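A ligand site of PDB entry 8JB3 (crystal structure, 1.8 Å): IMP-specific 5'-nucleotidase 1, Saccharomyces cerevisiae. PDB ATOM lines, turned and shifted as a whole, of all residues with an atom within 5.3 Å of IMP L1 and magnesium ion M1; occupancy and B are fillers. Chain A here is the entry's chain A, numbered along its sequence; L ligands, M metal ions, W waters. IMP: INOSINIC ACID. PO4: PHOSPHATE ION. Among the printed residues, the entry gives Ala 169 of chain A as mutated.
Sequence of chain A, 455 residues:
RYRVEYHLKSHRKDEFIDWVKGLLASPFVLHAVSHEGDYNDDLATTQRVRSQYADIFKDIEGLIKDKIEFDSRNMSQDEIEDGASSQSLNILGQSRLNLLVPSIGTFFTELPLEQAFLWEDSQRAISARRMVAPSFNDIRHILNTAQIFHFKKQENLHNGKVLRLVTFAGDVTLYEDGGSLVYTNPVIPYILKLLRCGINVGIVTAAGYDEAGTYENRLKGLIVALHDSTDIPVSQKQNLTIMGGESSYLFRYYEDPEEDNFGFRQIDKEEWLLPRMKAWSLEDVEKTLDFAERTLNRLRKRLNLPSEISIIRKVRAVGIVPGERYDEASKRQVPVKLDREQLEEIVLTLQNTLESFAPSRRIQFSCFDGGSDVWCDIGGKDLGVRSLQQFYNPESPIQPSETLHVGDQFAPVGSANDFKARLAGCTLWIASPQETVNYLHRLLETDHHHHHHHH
An oxygen (O2') of IMP L1 lies within hydrogen-bond range of the side-chain carboxylate (OD2) of Asp 171 (2.7 Å).
The side-chain hydroxyl of Tyr 209 is in hydrogen-bond range of an oxygen (O3P) of IMP L1.
The side-chain carboxylate (OD1) of Asp 377 lies within hydrogen-bond range of a nitrogen (N1) of IMP L1, 2.6 Å away.
NZ of Lys 314 is in hydrogen-bond range of N7 of IMP L1, at 2.9 Å.
O of Ala 206 is in hydrogen-bond range of N1 of IMP L1 (3.0 Å).
The indole nitrogen (NE1) of Trp 375 lies within hydrogen-bond range of an oxygen (O4') of IMP L1.
NH2 of Arg 218 lies within salt-bridge range of O1P of IMP L1, at 3.5 Å.
N of Gly 208 lies within hydrogen-bond range of N7 of IMP L1 (3.4 Å).
OD1 of Asp 171 is in salt-bridge range of NH1 of Arg 218, 2.9 Å away.
The side-chain carboxylate (OD1) of Asp 171 sits at hydrogen-bond distance from the backbone NH (N) of Gly 178.
The backbone NH (N) of Asp 408 sits at hydrogen-bond distance from the side-chain carboxylate (OD2) of Asp 418, at 3.1 Å.
The side-chain hydroxyl (OH) of Tyr 209 sits at hydrogen-bond distance from the guanidinium group (NH2) of Arg 218 (3.1 Å).
O of Gly 208 sits at hydrogen-bond distance from NZ of Lys 314, at 3.0 Å.
O of Trp 375 lies within hydrogen-bond range of N of Phe 368 (2.9 Å).
N of Ala 207 sits at hydrogen-bond distance from OG1 of Thr 205, at 3.1 Å.
N of Gly 245 lies within hydrogen-bond range of O of Ala 207.
The side-chain carboxylate (OD2) of Asp 373 sits close to an oxygen (O4') of IMP L1.
OD1 of Asp 177 touches O3' of IMP L1, 3.8 Å away.
CB of Ala 207 touches O2' of IMP L1 (3.3 Å).
Ala 317 touches IMP L1 (CB to O6, 3.5 Å).
Phe 368 touches IMP L1.
Hydrophobic or aromatic side chains that line IMP L1: Ala 206, Ala 207, Tyr 209, Ala 317, Phe 368 and Trp 375.
13 residues have an atom within 4 Å of IMP L1: Asp 171, Asp 177, Ala 206, Ala 207, Gly 208, Tyr 209, Arg 218, Lys 314, Ala 317, Phe 368, Asp 373, Trp 375 and Asp 377.
Along chain A the residues within 4 Å of IMP L1 span positions 171 to 377.
Merely in contact with magnesium ion M1: Ala 169 and Gln 409.
Four residues have an atom within 4 Å of magnesium ion M1: Ala 169, Asp 171, Asp 408 and Gln 409.
Water W2 binds magnesium ion M1 (2.1 Å).
O4 of PO4 L2 binds magnesium ion M1, at 2.1 Å.
Magnesium ion M1 is bound by O of Asp 171.
Magnesium ion M1 is bound by OD1 of Asp 408, at 2.3 Å.
Magnesium ion M1 is bound by water W7, 2.5 Å away.
Water W2 lies within hydrogen-bond range of the side-chain carboxylate of Asp 408 (2.8 Å) and the side-chain amide nitrogen of Gln 409 (2.9 Å).
Water W7 lies within hydrogen-bond range of OD2 of Asp 418 (2.5 Å), OD1 of Asn 417 (2.8 Å) and NZ of Lys 381 (3.2 Å).
Water W3 lies within hydrogen-bond range of O3' of IMP L1, OD1 of Asp 177 and N of Gly 178.
Water W8 lies within hydrogen-bond range of O1P of IMP L1 and O of Gly 178.
Water W4 lies within hydrogen-bond range of OD2 of Asp 373 (2.6 Å) and O3' of IMP L1 (2.8 Å).
Water W6 lies within hydrogen-bond range of the side-chain carboxylate (OD2) of Asp 171 (2.9 Å), the side-chain hydroxyl (OG1) of Thr 205 (3.0 Å), the guanidinium group (NH2) of Arg 218 (3.3 Å) and an oxygen (O2') of IMP L1 (3.5 Å).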
ATOM      1  N   ALA A 169      12.231 -14.440 -24.999  1.00  0.00           N
ATOM      2  CA  ALA A 169      13.570 -14.947 -24.706  1.00  0.00           C
ATOM      3  C   ALA A 169      13.764 -16.231 -25.544  1.00  0.00           C
ATOM      4  O   ALA A 169      12.800 -16.803 -26.082  1.00  0.00           O
ATOM      5  CB  ALA A 169      13.765 -15.224 -23.184  1.00  0.00           C
ATOM      6  N   GLY A 170      15.003 -16.700 -25.647  1.00  0.00           N
ATOM      7  CA  GLY A 170      15.256 -17.938 -26.361  1.00  0.00           C
ATOM      8  C   GLY A 170      15.346 -19.122 -25.422  1.00  0.00           C
ATOM      9  O   GLY A 170      14.462 -19.981 -25.360  1.00  0.00           O
ATOM     10  N   ASP A 171      16.441 -19.164 -24.677  1.00  0.00           N
ATOM     11  CA  ASP A 171      16.723 -20.252 -23.776  1.00  0.00           C
ATOM     12  C   ASP A 171      15.606 -20.378 -22.738  1.00  0.00           C
ATOM     13  O   ASP A 171      15.200 -19.385 -22.148  1.00  0.00           O
ATOM     14  CB  ASP A 171      18.064 -20.023 -23.087  1.00  0.00           C
ATOM     15  CG  ASP A 171      19.215 -19.951 -24.085  1.00  0.00           C
ATOM     16  OD1 ASP A 171      19.494 -20.981 -24.732  1.00  0.00           O
ATOM     17  OD2 ASP A 171      19.821 -18.869 -24.231  1.00  0.00           O
ATOM     18  N   VAL A 172      15.142 -21.618 -22.554  1.00  0.00           N
ATOM     19  CA  VAL A 172      14.113 -22.007 -21.573  1.00  0.00           C
ATOM     20  C   VAL A 172      12.732 -21.532 -22.046  1.00  0.00           C
ATOM     21  O   VAL A 172      11.717 -22.009 -21.572  1.00  0.00           O
ATOM     22  CB  VAL A 172      14.438 -21.492 -20.149  1.00  0.00           C
ATOM     23  CG1 VAL A 172      13.434 -22.058 -19.093  1.00  0.00           C
ATOM     24  CG2 VAL A 172      15.863 -21.870 -19.747  1.00  0.00           C
ATOM     25  N   THR A 173      12.687 -20.654 -23.021  1.00  0.00           N
ATOM     26  CA  THR A 173      11.412 -20.061 -23.424  1.00  0.00           C
ATOM     27  C   THR A 173      10.940 -20.672 -24.744  1.00  0.00           C
ATOM     28  O   THR A 173       9.785 -21.106 -24.869  1.00  0.00           O
ATOM     29  CB  THR A 173      11.541 -18.535 -23.556  1.00  0.00           C
ATOM     30  OG1 THR A 173      11.905 -17.973 -22.291  1.00  0.00           O
ATOM     31  CG2 THR A 173      10.213 -17.904 -24.052  1.00  0.00           C
ATOM     32  N   ASP A 177      17.421 -24.942 -22.442  1.00  0.00           N
ATOM     33  CA  ASP A 177      18.564 -24.061 -22.239  1.00  0.00           C
ATOM     34  C   ASP A 177      19.720 -24.505 -23.129  1.00  0.00           C
ATOM     35  O   ASP A 177      20.082 -25.676 -23.100  1.00  0.00           O
ATOM     36  CB  ASP A 177      18.958 -24.066 -20.754  1.00  0.00           C
ATOM     37  CG  ASP A 177      20.016 -23.053 -20.428  1.00  0.00           C
ATOM     38  OD1 ASP A 177      20.147 -22.073 -21.177  1.00  0.00           O
ATOM     39  OD2 ASP A 177      20.724 -23.254 -19.418  1.00  0.00           O
ATOM     40  N   GLY A 178      20.254 -23.579 -23.931  1.00  0.00           N
ATOM     41  CA  GLY A 178      21.366 -23.852 -24.828  1.00  0.00           C
ATOM     42  C   GLY A 178      20.956 -24.539 -26.114  1.00  0.00           C
ATOM     43  O   GLY A 178      21.802 -24.885 -26.958  1.00  0.00           O
ATOM     44  N   THR A 205      17.067 -12.080 -27.028  1.00  0.00           N
ATOM     45  CA  THR A 205      17.808 -13.142 -26.348  1.00  0.00           C
ATOM     46  C   THR A 205      19.182 -12.619 -25.966  1.00  0.00           C
ATOM     47  O   THR A 205      19.738 -11.773 -26.662  1.00  0.00           O
ATOM     48  CB  THR A 205      17.926 -14.396 -27.234  1.00  0.00           C
ATOM     49  OG1 THR A 205      18.797 -15.340 -26.615  1.00  0.00           O
ATOM     50  CG2 THR A 205      18.483 -14.035 -28.663  1.00  0.00           C
ATOM     51  N   ALA A 206      19.744 -13.112 -24.855  1.00  0.00           N
ATOM     52  CA  ALA A 206      21.070 -12.706 -24.482  1.00  0.00           C
ATOM     53  C   ALA A 206      22.104 -13.326 -25.451  1.00  0.00           C
ATOM     54  O   ALA A 206      23.211 -12.813 -25.536  1.00  0.00           O
ATOM     55  CB  ALA A 206      21.381 -13.117 -23.042  1.00  0.00           C
ATOM     56  N   ALA A 207      21.772 -14.446 -26.098  1.00  0.00           N
ATOM     57  CA  ALA A 207      22.689 -15.050 -27.087  1.00  0.00           C
ATOM     58  C   ALA A 207      23.090 -13.985 -28.099  1.00  0.00           C
ATOM     59  O   ALA A 207      22.221 -13.390 -28.733  1.00  0.00           O
ATOM     60  CB  ALA A 207      22.047 -16.242 -27.789  1.00  0.00           C
ATOM     61  N   GLY A 208      24.388 -13.709 -28.214  1.00  0.00           N
ATOM     62  CA  GLY A 208      24.872 -12.517 -28.905  1.00  0.00           C
ATOM     63  C   GLY A 208      25.852 -12.911 -30.008  1.00  0.00           C
ATOM     64  O   GLY A 208      27.007 -13.220 -29.735  1.00  0.00           O
ATOM     65  N   TYR A 209      25.381 -12.920 -31.252  1.00  0.00           N
ATOM     66  CA  TYR A 209      26.230 -13.281 -32.397  1.00  0.00           C
ATOM     67  C   TYR A 209      26.238 -12.164 -33.430  1.00  0.00           C
ATOM     68  O   TYR A 209      25.179 -11.708 -33.864  1.00  0.00           O
ATOM     69  CB  TYR A 209      25.745 -14.583 -33.047  1.00  0.00           C
ATOM     70  CG  TYR A 209      25.440 -15.663 -32.052  1.00  0.00           C
ATOM     71  CD1 TYR A 209      26.456 -16.224 -31.280  1.00  0.00           C
ATOM     72  CD2 TYR A 209      24.162 -16.139 -31.891  1.00  0.00           C
ATOM     73  CE1 TYR A 209      26.193 -17.199 -30.344  1.00  0.00           C
ATOM     74  CE2 TYR A 209      23.887 -17.141 -30.966  1.00  0.00           C
ATOM     75  CZ  TYR A 209      24.911 -17.669 -30.205  1.00  0.00           C
ATOM     76  OH  TYR A 209      24.664 -18.659 -29.258  1.00  0.00           O
ATOM     77  N   ARG A 218      20.345 -21.760 -34.964  1.00  0.00           N
ATOM     78  CA  ARG A 218      19.629 -22.003 -33.694  1.00  0.00           C
ATOM     79  C   ARG A 218      18.122 -21.833 -33.827  1.00  0.00           C
ATOM     80  O   ARG A 218      17.366 -22.350 -33.007  1.00  0.00           O
ATOM     81  CB  ARG A 218      20.154 -21.082 -32.587  1.00  0.00           C
ATOM     82  CG  ARG A 218      21.505 -21.526 -32.062  1.00  0.00           C
ATOM     83  CD  ARG A 218      21.886 -20.824 -30.781  1.00  0.00           C
ATOM     84  NE  ARG A 218      21.167 -21.357 -29.633  1.00  0.00           N
ATOM     85  CZ  ARG A 218      21.230 -20.841 -28.404  1.00  0.00           C
ATOM     86  NH1 ARG A 218      20.548 -21.389 -27.409  1.00  0.00           N
ATOM     87  NH2 ARG A 218      21.976 -19.749 -28.196  1.00  0.00           N
ATOM     88  N   GLY A 245      22.203 -10.454 -27.930  1.00  0.00           N
ATOM     89  CA  GLY A 245      23.024  -9.813 -26.927  1.00  0.00           C
ATOM     90  C   GLY A 245      22.191  -8.911 -26.037  1.00  0.00           C
ATOM     91  O   GLY A 245      22.725  -7.984 -25.438  1.00  0.00           O
ATOM     92  N   LYS A 314      33.454 -11.330 -25.503  1.00  0.00           N
ATOM     93  CA  LYS A 314      32.899 -10.931 -26.773  1.00  0.00           C
ATOM     94  C   LYS A 314      32.971  -9.404 -26.889  1.00  0.00           C
ATOM     95  O   LYS A 314      33.408  -8.704 -25.977  1.00  0.00           O
ATOM     96  CB  LYS A 314      31.441 -11.403 -26.922  1.00  0.00           C
ATOM     97  CG  LYS A 314      31.246 -12.936 -26.822  1.00  0.00           C
ATOM     98  CD  LYS A 314      29.863 -13.341 -27.297  1.00  0.00           C
ATOM     99  CE  LYS A 314      29.720 -14.842 -27.377  1.00  0.00           C
ATOM    100  NZ  LYS A 314      28.463 -15.222 -28.076  1.00  0.00           N
ATOM    101  N   ALA A 317      29.860  -8.518 -24.577  1.00  0.00           N
ATOM    102  CA  ALA A 317      29.530  -9.393 -23.445  1.00  0.00           C
ATOM    103  C   ALA A 317      30.787 -10.063 -22.937  1.00  0.00           C
ATOM    104  O   ALA A 317      31.774 -10.128 -23.673  1.00  0.00           O
ATOM    105  CB  ALA A 317      28.517 -10.443 -23.842  1.00  0.00           C
ATOM    106  N   VAL A 321      31.599 -20.202 -18.694  1.00  0.00           N
ATOM    107  CA  VAL A 321      30.743 -21.264 -19.142  1.00  0.00           C
ATOM    108  C   VAL A 321      31.319 -22.617 -18.803  1.00  0.00           C
ATOM    109  O   VAL A 321      32.519 -22.739 -18.548  1.00  0.00           O
ATOM    110  CB  VAL A 321      30.499 -21.178 -20.713  1.00  0.00           C
ATOM    111  CG1 VAL A 321      29.806 -19.880 -21.079  1.00  0.00           C
ATOM    112  CG2 VAL A 321      31.823 -21.293 -21.489  1.00  0.00           C
ATOM    113  N   PHE A 368      23.696 -11.978 -15.384  1.00  0.00           N
ATOM    114  CA  PHE A 368      22.737 -13.057 -15.087  1.00  0.00           C
ATOM    115  C   PHE A 368      23.398 -14.398 -14.986  1.00  0.00           C
ATOM    116  O   PHE A 368      24.474 -14.636 -15.522  1.00  0.00           O
ATOM    117  CB  PHE A 368      21.610 -13.094 -16.116  1.00  0.00           C
ATOM    118  CG  PHE A 368      22.057 -13.554 -17.500  1.00  0.00           C
ATOM    119  CD1 PHE A 368      22.053 -14.910 -17.826  1.00  0.00           C
ATOM    120  CD2 PHE A 368      22.502 -12.634 -18.447  1.00  0.00           C
ATOM    121  CE1 PHE A 368      22.445 -15.359 -19.074  1.00  0.00           C
ATOM    122  CE2 PHE A 368      22.911 -13.060 -19.707  1.00  0.00           C
ATOM    123  CZ  PHE A 368      22.875 -14.424 -20.033  1.00  0.00           C
ATOM    124  N   ASP A 373      25.683 -21.081 -16.441  1.00  0.00           N
ATOM    125  CA  ASP A 373      26.690 -20.099 -16.779  1.00  0.00           C
ATOM    126  C   ASP A 373      26.337 -18.751 -16.176  1.00  0.00           C
ATOM    127  O   ASP A 373      25.221 -18.562 -15.674  1.00  0.00           O
ATOM    128  CB  ASP A 373      26.851 -19.975 -18.316  1.00  0.00           C
ATOM    129  CG  ASP A 373      25.543 -19.650 -19.037  1.00  0.00           C
ATOM    130  OD1 ASP A 373      24.546 -19.315 -18.381  1.00  0.00           O
ATOM    131  OD2 ASP A 373      25.491 -19.763 -20.266  1.00  0.00           O
ATOM    132  N   TRP A 375      26.769 -14.561 -17.375  1.00  0.00           N
ATOM    133  CA  TRP A 375      27.193 -13.541 -18.337  1.00  0.00           C
ATOM    134  C   TRP A 375      26.940 -12.106 -17.866  1.00  0.00           C
ATOM    135  O   TRP A 375      25.999 -11.808 -17.127  1.00  0.00           O
ATOM    136  CB  TRP A 375      26.469 -13.721 -19.675  1.00  0.00           C
ATOM    137  CG  TRP A 375      26.813 -14.951 -20.413  1.00  0.00           C
ATOM    138  CD1 TRP A 375      26.288 -16.203 -20.240  1.00  0.00           C
ATOM    139  CD2 TRP A 375      27.750 -15.046 -21.492  1.00  0.00           C
ATOM    140  NE1 TRP A 375      26.858 -17.076 -21.149  1.00  0.00           N
ATOM    141  CE2 TRP A 375      27.766 -16.387 -21.926  1.00  0.00           C
ATOM    142  CE3 TRP A 375      28.591 -14.113 -22.147  1.00  0.00           C
ATOM    143  CZ2 TRP A 375      28.582 -16.837 -22.995  1.00  0.00           C
ATOM    144  CZ3 TRP A 375      29.407 -14.554 -23.213  1.00  0.00           C
ATOM    145  CH2 TRP A 375      29.404 -15.902 -23.612  1.00  0.00           C
ATOM    146  N   ASP A 377      26.247  -8.748 -20.064  1.00  0.00           N
ATOM    147  CA  ASP A 377      25.983  -8.077 -21.323  1.00  0.00           C
ATOM    148  C   ASP A 377      25.958  -6.581 -21.166  1.00  0.00           C
ATOM    149  O   ASP A 377      25.411  -6.065 -20.205  1.00  0.00           O
ATOM    150  CB  ASP A 377      24.627  -8.453 -21.922  1.00  0.00           C
ATOM    151  CG  ASP A 377      24.611  -9.864 -22.435  1.00  0.00           C
ATOM    152  OD1 ASP A 377      25.581 -10.238 -23.131  1.00  0.00           O
ATOM    153  OD2 ASP A 377      23.654 -10.609 -22.145  1.00  0.00           O
ATOM    154  N   LYS A 381      17.455  -6.010 -21.732  1.00  0.00           N
ATOM    155  CA  LYS A 381      16.314  -6.317 -22.593  1.00  0.00           C
ATOM    156  C   LYS A 381      15.266  -5.233 -22.569  1.00  0.00           C
ATOM    157  O   LYS A 381      14.379  -5.225 -23.452  1.00  0.00           O
ATOM    158  CB  LYS A 381      15.687  -7.684 -22.220  1.00  0.00           C
ATOM    159  CG  LYS A 381      16.628  -8.860 -22.490  1.00  0.00           C
ATOM    160  CD  LYS A 381      15.885 -10.201 -22.499  1.00  0.00           C
ATOM    161  CE  LYS A 381      16.876 -11.365 -22.633  1.00  0.00           C
ATOM    162  NZ  LYS A 381      16.192 -12.731 -22.683  1.00  0.00           N
ATOM    163  N   ASP A 408      11.867 -16.198 -18.877  1.00  0.00           N
ATOM    164  CA  ASP A 408      11.929 -16.999 -17.643  1.00  0.00           C
ATOM    165  C   ASP A 408      12.758 -16.326 -16.567  1.00  0.00           C
ATOM    166  O   ASP A 408      12.648 -16.671 -15.396  1.00  0.00           O
ATOM    167  CB  ASP A 408      12.510 -18.412 -17.915  1.00  0.00           C
ATOM    168  CG  ASP A 408      13.948 -18.358 -18.425  1.00  0.00           C
ATOM    169  OD1 ASP A 408      14.163 -17.672 -19.431  1.00  0.00           O
ATOM    170  OD2 ASP A 408      14.851 -18.963 -17.804  1.00  0.00           O
ATOM    171  N   GLN A 409      13.570 -15.326 -16.948  1.00  0.00           N
ATOM    172  CA  GLN A 409      14.533 -14.772 -16.019  1.00  0.00           C
ATOM    173  C   GLN A 409      14.016 -13.507 -15.399  1.00  0.00           C
ATOM    174  O   GLN A 409      14.512 -12.413 -15.713  1.00  0.00           O
ATOM    175  CB  GLN A 409      15.878 -14.522 -16.693  1.00  0.00           C
ATOM    176  CG  GLN A 409      16.552 -15.790 -17.117  1.00  0.00           C
ATOM    177  CD  GLN A 409      17.991 -15.530 -17.503  1.00  0.00           C
ATOM    178  OE1 GLN A 409      18.577 -14.579 -17.012  1.00  0.00           O
ATOM    179  NE2 GLN A 409      18.544 -16.354 -18.395  1.00  0.00           N
ATOM    180  N   ASN A 417      17.829 -11.765 -16.530  1.00  0.00           N
ATOM    181  CA  ASN A 417      18.055 -10.944 -17.737  1.00  0.00           C
ATOM    182  C   ASN A 417      16.763 -10.553 -18.438  1.00  0.00           C
ATOM    183  O   ASN A 417      16.792  -9.796 -19.408  1.00  0.00           O
ATOM    184  CB  ASN A 417      19.033 -11.644 -18.740  1.00  0.00           C
ATOM    185  CG  ASN A 417      18.421 -12.776 -19.559  1.00  0.00           C
ATOM    186  OD1 ASN A 417      17.204 -12.963 -19.656  1.00  0.00           O
ATOM    187  ND2 ASN A 417      19.307 -13.521 -20.237  1.00  0.00           N
ATOM    188  N   ASP A 418      15.618 -11.042 -17.952  1.00  0.00           N
ATOM    189  CA  ASP A 418      14.332 -10.610 -18.492  1.00  0.00           C
ATOM    190  C   ASP A 418      13.684  -9.554 -17.618  1.00  0.00           C
ATOM    191  O   ASP A 418      12.750  -8.893 -18.043  1.00  0.00           O
ATOM    192  CB  ASP A 418      13.383 -11.789 -18.653  1.00  0.00           C
ATOM    193  CG  ASP A 418      13.828 -12.761 -19.740  1.00  0.00           C
ATOM    194  OD1 ASP A 418      14.118 -12.302 -20.894  1.00  0.00           O
ATOM    195  OD2 ASP A 418      13.890 -13.985 -19.438  1.00  0.00           O
HETATM  196  P   IMP L   1      26.299 -20.888 -27.223  1.00  0.00           P
HETATM  197  O1P IMP L   1      24.954 -21.515 -27.577  1.00  0.00           O
HETATM  198  O2P IMP L   1      27.450 -21.855 -26.932  1.00  0.00           O
HETATM  199  O3P IMP L   1      26.625 -19.918 -28.323  1.00  0.00           O
HETATM  200  O5' IMP L   1      26.127 -20.008 -25.916  1.00  0.00           O
HETATM  201  C5' IMP L   1      26.253 -20.572 -24.619  1.00  0.00           C
HETATM  202  C4' IMP L   1      25.167 -20.046 -23.710  1.00  0.00           C
HETATM  203  O4' IMP L   1      25.405 -18.641 -23.452  1.00  0.00           O
HETATM  204  C3' IMP L   1      23.781 -20.140 -24.305  1.00  0.00           C
HETATM  205  O3' IMP L   1      22.812 -20.240 -23.260  1.00  0.00           O
HETATM  206  C2' IMP L   1      23.630 -18.815 -25.006  1.00  0.00           C
HETATM  207  O2' IMP L   1      22.288 -18.472 -25.305  1.00  0.00           O
HETATM  208  C1' IMP L   1      24.387 -17.857 -24.044  1.00  0.00           C
HETATM  209  N9  IMP L   1      25.093 -16.770 -24.726  1.00  0.00           N
HETATM  210  C8  IMP L   1      25.786 -16.876 -25.880  1.00  0.00           C
HETATM  211  N7  IMP L   1      26.306 -15.655 -26.211  1.00  0.00           N
HETATM  212  C5  IMP L   1      25.940 -14.792 -25.212  1.00  0.00           C
HETATM  213  C6  IMP L   1      26.191 -13.341 -25.015  1.00  0.00           C
HETATM  214  O6  IMP L   1      26.819 -12.709 -25.835  1.00  0.00           O
HETATM  215  N1  IMP L   1      25.660 -12.696 -23.837  1.00  0.00           N
HETATM  216  C2  IMP L   1      24.905 -13.436 -22.876  1.00  0.00           C
HETATM  217  N3  IMP L   1      24.671 -14.820 -23.096  1.00  0.00           N
HETATM  218  C4  IMP L   1      25.217 -15.490 -24.307  1.00  0.00           C
HETATM  219  P   PO4 L   2      18.130 -15.964 -23.207  1.00  0.00           P
HETATM  220  O1  PO4 L   2      17.444 -16.320 -24.478  1.00  0.00           O
HETATM  221  O2  PO4 L   2      18.184 -14.487 -22.923  1.00  0.00           O
HETATM  222  O3  PO4 L   2      19.539 -16.480 -23.227  1.00  0.00           O
HETATM  223  O4  PO4 L   2      17.495 -16.691 -22.058  1.00  0.00           O
HETATM  224 MG    MG M   1      15.874 -17.577 -20.994  1.00  0.00          MG
HETATM  225 MG    MG M   2      28.837 -18.148 -27.637  1.00  0.00          MG
HETATM  226  O   HOH W   1      26.855 -10.136 -27.056  1.00  0.00           O
HETATM  227  O   HOH W   2      16.999 -18.590 -19.514  1.00  0.00           O
HETATM  228  O   HOH W   3      22.783 -22.261 -21.931  1.00  0.00           O
HETATM  229  O   HOH W   4      23.065 -18.947 -20.811  1.00  0.00           O
HETATM  230  O   HOH W   5      27.314 -20.880 -30.895  1.00  0.00           O
HETATM  231  O   HOH W   6      19.253 -18.256 -26.963  1.00  0.00           O
HETATM  232  O   HOH W   7      15.822 -15.143 -20.605  1.00  0.00           O
HETATM  233  O   HOH W   8      24.389 -24.035 -26.737  1.00  0.00           O
